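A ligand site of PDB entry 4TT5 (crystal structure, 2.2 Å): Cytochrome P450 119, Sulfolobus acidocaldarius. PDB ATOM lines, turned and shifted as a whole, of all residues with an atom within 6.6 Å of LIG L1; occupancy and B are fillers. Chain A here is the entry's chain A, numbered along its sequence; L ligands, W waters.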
ATOM      1  N   LEU A  69     -20.776 -13.453  16.133  1.00  0.00           N
ATOM      2  CA  LEU A  69     -19.645 -13.432  15.201  1.00  0.00           C
ATOM      3  C   LEU A  69     -18.575 -12.434  15.647  1.00  0.00           C
ATOM      4  O   LEU A  69     -17.375 -12.686  15.493  1.00  0.00           O
ATOM      5  CB  LEU A  69     -20.127 -13.075  13.778  1.00  0.00           C
ATOM      6  CG  LEU A  69     -19.086 -13.071  12.673  1.00  0.00           C
ATOM      7  CD1 LEU A  69     -18.525 -14.485  12.428  1.00  0.00           C
ATOM      8  CD2 LEU A  69     -19.672 -12.493  11.387  1.00  0.00           C
ATOM      9  N   VAL A 151     -24.488  -9.123   1.865  1.00  0.00           N
ATOM     10  CA  VAL A 151     -23.355  -9.590   2.657  1.00  0.00           C
ATOM     11  C   VAL A 151     -22.064  -9.297   1.896  1.00  0.00           C
ATOM     12  O   VAL A 151     -21.950  -9.621   0.711  1.00  0.00           O
ATOM     13  CB  VAL A 151     -23.513 -11.100   3.046  1.00  0.00           C
ATOM     14  CG1 VAL A 151     -23.168 -12.035   1.873  1.00  0.00           C
ATOM     15  CG2 VAL A 151     -22.687 -11.424   4.240  1.00  0.00           C
ATOM     16  N   ALA A 152     -21.113  -8.652   2.562  1.00  0.00           N
ATOM     17  CA  ALA A 152     -19.876  -8.230   1.888  1.00  0.00           C
ATOM     18  C   ALA A 152     -18.795  -7.786   2.856  1.00  0.00           C
ATOM     19  O   ALA A 152     -19.078  -7.302   3.954  1.00  0.00           O
ATOM     20  CB  ALA A 152     -20.166  -7.085   0.885  1.00  0.00           C
ATOM     21  N   PHE A 153     -17.544  -7.925   2.441  1.00  0.00           N
ATOM     22  CA  PHE A 153     -16.465  -7.250   3.132  1.00  0.00           C
ATOM     23  C   PHE A 153     -16.711  -5.740   3.075  1.00  0.00           C
ATOM     24  O   PHE A 153     -17.061  -5.203   2.020  1.00  0.00           O
ATOM     25  CB  PHE A 153     -15.115  -7.608   2.515  1.00  0.00           C
ATOM     26  CG  PHE A 153     -13.980  -6.809   3.074  1.00  0.00           C
ATOM     27  CD1 PHE A 153     -13.512  -7.053   4.355  1.00  0.00           C
ATOM     28  CD2 PHE A 153     -13.378  -5.798   2.320  1.00  0.00           C
ATOM     29  CE1 PHE A 153     -12.462  -6.309   4.886  1.00  0.00           C
ATOM     30  CE2 PHE A 153     -12.334  -5.066   2.830  1.00  0.00           C
ATOM     31  CZ  PHE A 153     -11.877  -5.313   4.120  1.00  0.00           C
ATOM     32  N   ARG A 154     -16.542  -5.059   4.201  1.00  0.00           N
ATOM     33  CA  ARG A 154     -16.787  -3.621   4.246  1.00  0.00           C
ATOM     34  C   ARG A 154     -15.526  -2.861   4.685  1.00  0.00           C
ATOM     35  O   ARG A 154     -15.249  -2.753   5.885  1.00  0.00           O
ATOM     36  CB  ARG A 154     -17.957  -3.293   5.174  1.00  0.00           C
ATOM     37  CG  ARG A 154     -19.236  -4.105   4.915  1.00  0.00           C
ATOM     38  CD  ARG A 154     -19.645  -4.042   3.444  1.00  0.00           C
ATOM     39  NE  ARG A 154     -20.031  -2.692   3.028  1.00  0.00           N
ATOM     40  CZ  ARG A 154     -19.782  -2.183   1.824  1.00  0.00           C
ATOM     41  NH1 ARG A 154     -19.141  -2.897   0.917  1.00  0.00           N
ATOM     42  NH2 ARG A 154     -20.187  -0.947   1.537  1.00  0.00           N
ATOM     43  N   GLU A 160     -17.903  -5.559  10.338  1.00  0.00           N
ATOM     44  CA  GLU A 160     -19.163  -5.365   9.623  1.00  0.00           C
ATOM     45  C   GLU A 160     -19.201  -6.133   8.294  1.00  0.00           C
ATOM     46  O   GLU A 160     -18.362  -5.909   7.431  1.00  0.00           O
ATOM     47  CB  GLU A 160     -19.435  -3.878   9.360  1.00  0.00           C
ATOM     48  CG  GLU A 160     -19.712  -3.026  10.597  1.00  0.00           C
ATOM     49  CD  GLU A 160     -20.565  -1.791  10.296  1.00  0.00           C
ATOM     50  OE1 GLU A 160     -21.207  -1.740   9.221  1.00  0.00           O
ATOM     51  OE2 GLU A 160     -20.605  -0.867  11.127  1.00  0.00           O
ATOM     52  N   ILE A 161     -20.182  -7.015   8.125  1.00  0.00           N
ATOM     53  CA  ILE A 161     -20.283  -7.780   6.878  1.00  0.00           C
ATOM     54  C   ILE A 161     -21.583  -7.527   6.100  1.00  0.00           C
ATOM     55  O   ILE A 161     -21.960  -8.311   5.225  1.00  0.00           O
ATOM     56  CB  ILE A 161     -20.149  -9.295   7.147  1.00  0.00           C
ATOM     57  CG1 ILE A 161     -21.292  -9.786   8.045  1.00  0.00           C
ATOM     58  CG2 ILE A 161     -18.792  -9.614   7.778  1.00  0.00           C
ATOM     59  CD1 ILE A 161     -21.406 -11.291   8.145  1.00  0.00           C
ATOM     60  N   LEU A 205     -28.554 -12.425  11.299  1.00  0.00           N
ATOM     61  CA  LEU A 205     -27.403 -13.292  11.092  1.00  0.00           C
ATOM     62  C   LEU A 205     -27.840 -14.705  10.677  1.00  0.00           C
ATOM     63  O   LEU A 205     -27.342 -15.264   9.698  1.00  0.00           O
ATOM     64  CB  LEU A 205     -26.564 -13.345  12.370  1.00  0.00           C
ATOM     65  CG  LEU A 205     -25.230 -14.087  12.290  1.00  0.00           C
ATOM     66  CD1 LEU A 205     -24.186 -13.255  11.551  1.00  0.00           C
ATOM     67  CD2 LEU A 205     -24.759 -14.439  13.694  1.00  0.00           C
ATOM     68  N   ILE A 208     -29.910 -14.625   7.045  1.00  0.00           N
ATOM     69  CA  ILE A 208     -29.313 -14.079   5.830  1.00  0.00           C
ATOM     70  C   ILE A 208     -27.835 -14.427   5.626  1.00  0.00           C
ATOM     71  O   ILE A 208     -27.410 -14.679   4.505  1.00  0.00           O
ATOM     72  CB  ILE A 208     -29.483 -12.530   5.819  1.00  0.00           C
ATOM     73  CG1 ILE A 208     -30.957 -12.160   5.891  1.00  0.00           C
ATOM     74  CG2 ILE A 208     -28.870 -11.900   4.563  1.00  0.00           C
ATOM     75  CD1 ILE A 208     -31.798 -12.744   4.772  1.00  0.00           C
ATOM     76  N   ALA A 209     -27.072 -14.497   6.712  1.00  0.00           N
ATOM     77  CA  ALA A 209     -25.613 -14.480   6.601  1.00  0.00           C
ATOM     78  C   ALA A 209     -25.057 -15.738   5.963  1.00  0.00           C
ATOM     79  O   ALA A 209     -23.963 -15.698   5.407  1.00  0.00           O
ATOM     80  CB  ALA A 209     -24.977 -14.279   7.970  1.00  0.00           C
ATOM     81  N   GLY A 210     -25.803 -16.829   6.032  1.00  0.00           N
ATOM     82  CA  GLY A 210     -25.345 -18.093   5.479  1.00  0.00           C
ATOM     83  C   GLY A 210     -25.785 -18.428   4.059  1.00  0.00           C
ATOM     84  O   GLY A 210     -25.368 -19.446   3.509  1.00  0.00           O
ATOM     85  N   ASN A 211     -26.602 -17.580   3.441  1.00  0.00           N
ATOM     86  CA  ASN A 211     -27.160 -17.939   2.131  1.00  0.00           C
ATOM     87  C   ASN A 211     -26.139 -17.926   0.987  1.00  0.00           C
ATOM     88  O   ASN A 211     -25.952 -18.943   0.293  1.00  0.00           O
ATOM     89  CB  ASN A 211     -28.335 -17.019   1.812  1.00  0.00           C
ATOM     90  CG  ASN A 211     -29.442 -17.159   2.832  1.00  0.00           C
ATOM     91  OD1 ASN A 211     -29.634 -18.236   3.392  1.00  0.00           O
ATOM     92  ND2 ASN A 211     -30.147 -16.080   3.106  1.00  0.00           N
ATOM     93  N   THR A 213     -22.871 -17.897   1.119  1.00  0.00           N
ATOM     94  CA  THR A 213     -21.735 -18.795   1.324  1.00  0.00           C
ATOM     95  C   THR A 213     -22.099 -20.214   0.920  1.00  0.00           C
ATOM     96  O   THR A 213     -21.296 -20.932   0.314  1.00  0.00           O
ATOM     97  CB  THR A 213     -21.232 -18.805   2.793  1.00  0.00           C
ATOM     98  OG1 THR A 213     -22.343 -18.984   3.676  1.00  0.00           O
ATOM     99  CG2 THR A 213     -20.549 -17.465   3.143  1.00  0.00           C
ATOM    100  N   VAL A 254     -15.441 -18.676   1.856  1.00  0.00           N
ATOM    101  CA  VAL A 254     -14.923 -17.566   2.643  1.00  0.00           C
ATOM    102  C   VAL A 254     -13.401 -17.664   2.610  1.00  0.00           C
ATOM    103  O   VAL A 254     -12.827 -18.614   3.160  1.00  0.00           O
ATOM    104  CB  VAL A 254     -15.452 -17.568   4.083  1.00  0.00           C
ATOM    105  CG1 VAL A 254     -14.967 -16.328   4.857  1.00  0.00           C
ATOM    106  CG2 VAL A 254     -16.951 -17.612   4.095  1.00  0.00           C
ATOM    107  N   ARG A 256     -11.034 -15.806   3.844  1.00  0.00           N
ATOM    108  CA  ARG A 256     -10.246 -15.312   4.954  1.00  0.00           C
ATOM    109  C   ARG A 256     -11.140 -14.744   6.044  1.00  0.00           C
ATOM    110  O   ARG A 256     -12.325 -14.469   5.814  1.00  0.00           O
ATOM    111  CB  ARG A 256      -9.286 -14.225   4.464  1.00  0.00           C
ATOM    112  CG  ARG A 256      -9.922 -12.877   4.421  1.00  0.00           C
ATOM    113  CD  ARG A 256      -9.227 -11.939   3.502  1.00  0.00           C
ATOM    114  NE  ARG A 256      -9.859 -10.629   3.604  1.00  0.00           N
ATOM    115  CZ  ARG A 256      -9.698  -9.646   2.731  1.00  0.00           C
ATOM    116  NH1 ARG A 256      -8.931  -9.825   1.675  1.00  0.00           N
ATOM    117  NH2 ARG A 256     -10.321  -8.494   2.925  1.00  0.00           N
ATOM    118  N   THR A 257     -10.577 -14.560   7.235  1.00  0.00           N
ATOM    119  CA  THR A 257     -11.253 -13.823   8.297  1.00  0.00           C
ATOM    120  C   THR A 257     -10.217 -12.982   9.037  1.00  0.00           C
ATOM    121  O   THR A 257      -9.048 -12.934   8.629  1.00  0.00           O
ATOM    122  CB  THR A 257     -12.041 -14.768   9.255  1.00  0.00           C
ATOM    123  OG1 THR A 257     -12.814 -13.980  10.175  1.00  0.00           O
ATOM    124  CG2 THR A 257     -11.104 -15.685  10.009  1.00  0.00           C
ATOM    125  N   CYS A 317     -17.902 -22.460  12.236  1.00  0.00           N
ATOM    126  CA  CYS A 317     -19.175 -22.070  11.649  1.00  0.00           C
ATOM    127  C   CYS A 317     -20.380 -22.800  12.240  1.00  0.00           C
ATOM    128  O   CYS A 317     -20.480 -24.015  12.147  1.00  0.00           O
ATOM    129  CB  CYS A 317     -19.169 -22.284  10.126  1.00  0.00           C
ATOM    130  SG  CYS A 317     -20.774 -21.917   9.377  1.00  0.00           S
ATOM    131  N   LEU A 318     -21.293 -22.023  12.817  1.00  0.00           N
ATOM    132  CA  LEU A 318     -22.554 -22.566  13.328  1.00  0.00           C
ATOM    133  C   LEU A 318     -23.340 -23.305  12.246  1.00  0.00           C
ATOM    134  O   LEU A 318     -24.042 -24.281  12.538  1.00  0.00           O
ATOM    135  CB  LEU A 318     -23.419 -21.445  13.915  1.00  0.00           C
ATOM    136  CG  LEU A 318     -24.769 -21.809  14.545  1.00  0.00           C
ATOM    137  CD1 LEU A 318     -24.570 -22.823  15.683  1.00  0.00           C
ATOM    138  CD2 LEU A 318     -25.512 -20.557  15.049  1.00  0.00           C
ATOM    139  N   GLY A 319     -23.246 -22.849  10.995  1.00  0.00           N
ATOM    140  CA  GLY A 319     -24.005 -23.464   9.927  1.00  0.00           C
ATOM    141  C   GLY A 319     -23.289 -24.587   9.183  1.00  0.00           C
ATOM    142  O   GLY A 319     -23.792 -25.084   8.180  1.00  0.00           O
ATOM    143  N   VAL A 353     -13.819 -11.185  -0.053  1.00  0.00           N
ATOM    144  CA  VAL A 353     -13.806 -12.281   0.906  1.00  0.00           C
ATOM    145  C   VAL A 353     -14.605 -13.478   0.404  1.00  0.00           C
ATOM    146  O   VAL A 353     -14.199 -14.618   0.588  1.00  0.00           O
ATOM    147  CB  VAL A 353     -14.341 -11.804   2.282  1.00  0.00           C
ATOM    148  CG1 VAL A 353     -14.527 -12.988   3.221  1.00  0.00           C
ATOM    149  CG2 VAL A 353     -13.393 -10.750   2.877  1.00  0.00           C
ATOM    150  N   LEU A 354     -15.736 -13.200  -0.220  1.00  0.00           N
ATOM    151  CA  LEU A 354     -16.582 -14.246  -0.754  1.00  0.00           C
ATOM    152  C   LEU A 354     -16.084 -14.727  -2.106  1.00  0.00           C
ATOM    153  O   LEU A 354     -15.749 -13.932  -2.996  1.00  0.00           O
ATOM    154  CB  LEU A 354     -18.018 -13.761  -0.852  1.00  0.00           C
ATOM    155  CG  LEU A 354     -18.536 -13.290   0.498  1.00  0.00           C
ATOM    156  CD1 LEU A 354     -19.880 -12.647   0.324  1.00  0.00           C
ATOM    157  CD2 LEU A 354     -18.612 -14.484   1.451  1.00  0.00           C
HETATM  158  C1  LIG L   1     -21.831 -17.475   7.272  1.00  0.00           C
HETATM  159  C2  LIG L   1     -20.260 -16.030   6.762  1.00  0.00           C
HETATM  160  C3  LIG L   1     -19.685 -17.092   7.472  1.00  0.00           C
HETATM  161  C4  LIG L   1     -19.568 -14.806   6.181  1.00  0.00           C
HETATM  162  C5  LIG L   1     -18.236 -14.499   6.440  1.00  0.00           C
HETATM  163  C6  LIG L   1     -17.634 -13.374   5.853  1.00  0.00           C
HETATM  164  C7  LIG L   1     -18.370 -12.550   5.002  1.00  0.00           C
HETATM  165  C8  LIG L   1     -19.691 -12.879   4.748  1.00  0.00           C
HETATM  166 BR1  LIG L   1     -17.632 -10.988   4.154  1.00  0.00          BR
HETATM  167  C9  LIG L   1     -20.295 -13.992   5.327  1.00  0.00           C
HETATM  168  N1  LIG L   1     -20.686 -17.950   7.768  1.00  0.00           N
HETATM  169  N2  LIG L   1     -21.581 -16.314   6.653  1.00  0.00           N
HETATM  170  C1  LG2 L   2     -19.072 -18.562  11.204  1.00  0.00           C
HETATM  171  C2  LG2 L   2     -17.824 -20.135   6.753  1.00  0.00           C
HETATM  172  C3  LG2 L   2     -22.463 -21.381   6.027  1.00  0.00           C
HETATM  173  C4  LG2 L   2     -23.738 -19.008  10.056  1.00  0.00           C
HETATM  174  C5  LG2 L   2     -18.328 -18.921  10.081  1.00  0.00           C
HETATM  175  C6  LG2 L   2     -16.897 -18.821   9.948  1.00  0.00           C
HETATM  176  C7  LG2 L   2     -16.569 -19.238   8.721  1.00  0.00           C
HETATM  177  C8  LG2 L   2     -17.781 -19.631   8.036  1.00  0.00           C
HETATM  178  C9  LG2 L   2     -15.171 -19.317   8.114  1.00  0.00           C
HETATM  179  C10 LG2 L   2     -15.900 -18.310  11.025  1.00  0.00           C
HETATM  180  C11 LG2 L   2     -15.716 -16.786  10.980  1.00  0.00           C
HETATM  181  C12 LG2 L   2     -14.723 -16.401  12.066  1.00  0.00           C
HETATM  182  O1  LG2 L   2     -14.072 -17.283  12.683  1.00  0.00           O
HETATM  183  O2  LG2 L   2     -14.561 -15.181  12.303  1.00  0.00           O
HETATM  184  C13 LG2 L   2     -18.964 -20.684   6.173  1.00  0.00           C
HETATM  185  C14 LG2 L   2     -19.036 -21.418   4.933  1.00  0.00           C
HETATM  186  C15 LG2 L   2     -20.333 -21.755   4.731  1.00  0.00           C
HETATM  187  C16 LG2 L   2     -21.101 -21.235   5.839  1.00  0.00           C
HETATM  188  C17 LG2 L   2     -17.806 -21.734   4.048  1.00  0.00           C
HETATM  189  C18 LG2 L   2     -20.987 -22.566   3.585  1.00  0.00           C
HETATM  190  C19 LG2 L   2     -20.302 -23.344   2.732  1.00  0.00           C
HETATM  191  C20 LG2 L   2     -23.223 -20.859   7.053  1.00  0.00           C
HETATM  192  C21 LG2 L   2     -24.665 -20.990   7.247  1.00  0.00           C
HETATM  193  C22 LG2 L   2     -24.987 -20.313   8.356  1.00  0.00           C
HETATM  194  C23 LG2 L   2     -23.771 -19.756   8.901  1.00  0.00           C
HETATM  195  C24 LG2 L   2     -25.621 -21.768   6.312  1.00  0.00           C
HETATM  196  C25 LG2 L   2     -26.344 -20.059   9.077  1.00  0.00           C
HETATM  197  C26 LG2 L   2     -27.503 -20.644   8.802  1.00  0.00           C
HETATM  198  C27 LG2 L   2     -22.594 -18.711  10.766  1.00  0.00           C
HETATM  199  C28 LG2 L   2     -22.544 -18.125  12.092  1.00  0.00           C
HETATM  200  C29 LG2 L   2     -21.253 -17.993  12.419  1.00  0.00           C
HETATM  201  C30 LG2 L   2     -20.448 -18.505  11.309  1.00  0.00           C
HETATM  202  C31 LG2 L   2     -23.812 -17.741  12.899  1.00  0.00           C
HETATM  203  C32 LG2 L   2     -20.728 -17.417  13.752  1.00  0.00           C
HETATM  204  C33 LG2 L   2     -20.369 -18.565  14.701  1.00  0.00           C
HETATM  205  C34 LG2 L   2     -19.760 -18.018  15.975  1.00  0.00           C
HETATM  206  O3  LG2 L   2     -19.272 -16.848  16.011  1.00  0.00           O
HETATM  207  O4  LG2 L   2     -19.716 -18.763  16.971  1.00  0.00           O
HETATM  208  N1  LG2 L   2     -18.830 -19.430   8.903  1.00  0.00           N
HETATM  209  N2  LG2 L   2     -20.231 -20.590   6.680  1.00  0.00           N
HETATM  210  N3  LG2 L   2     -22.715 -20.095   8.091  1.00  0.00           N
HETATM  211  N4  LG2 L   2     -21.308 -18.911  10.327  1.00  0.00           N
HETATM  212 FE1  LG2 L   2     -20.786 -19.786   8.522  1.00  0.00          FE
HETATM  213  O   HOH W   1     -14.383 -13.075   6.984  1.00  0.00           O
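O of Ala 209 sits at hydrogen-bond distance from N2 of LIG L1 (2.8 Å).
FE1 of LG2 L2 is bound by SG of Cys 317 (2.3 Å).
The side-chain hydroxyl (OG1) of Thr 257 sits at hydrogen-bond distance from an oxygen (O2) of LG2 L2.
FE1 of LG2 L2 is bound by N1 of LIG L1, at 2.0 Å.
The backbone NH (N) of Ala 152 lies within hydrogen-bond range of the backbone carbonyl oxygen (O) of Ile 161.
The side-chain hydroxyl of Thr 213 sits at hydrogen-bond distance from the backbone carbonyl oxygen of Gly 210.
Merely in contact with LIG L1: Val 151, Phe 153, Ala 152, Val 353, Leu 354, Thr 213 and Gly 210.
Within 4 Å of LIG L1: Val 151, Ala 152, Phe 153, Ala 209, Gly 210, Thr 213, Val 353 and Leu 354.
The nearest printed residue that does not touch LIG L1 is Ile 161 (4.05 Å).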
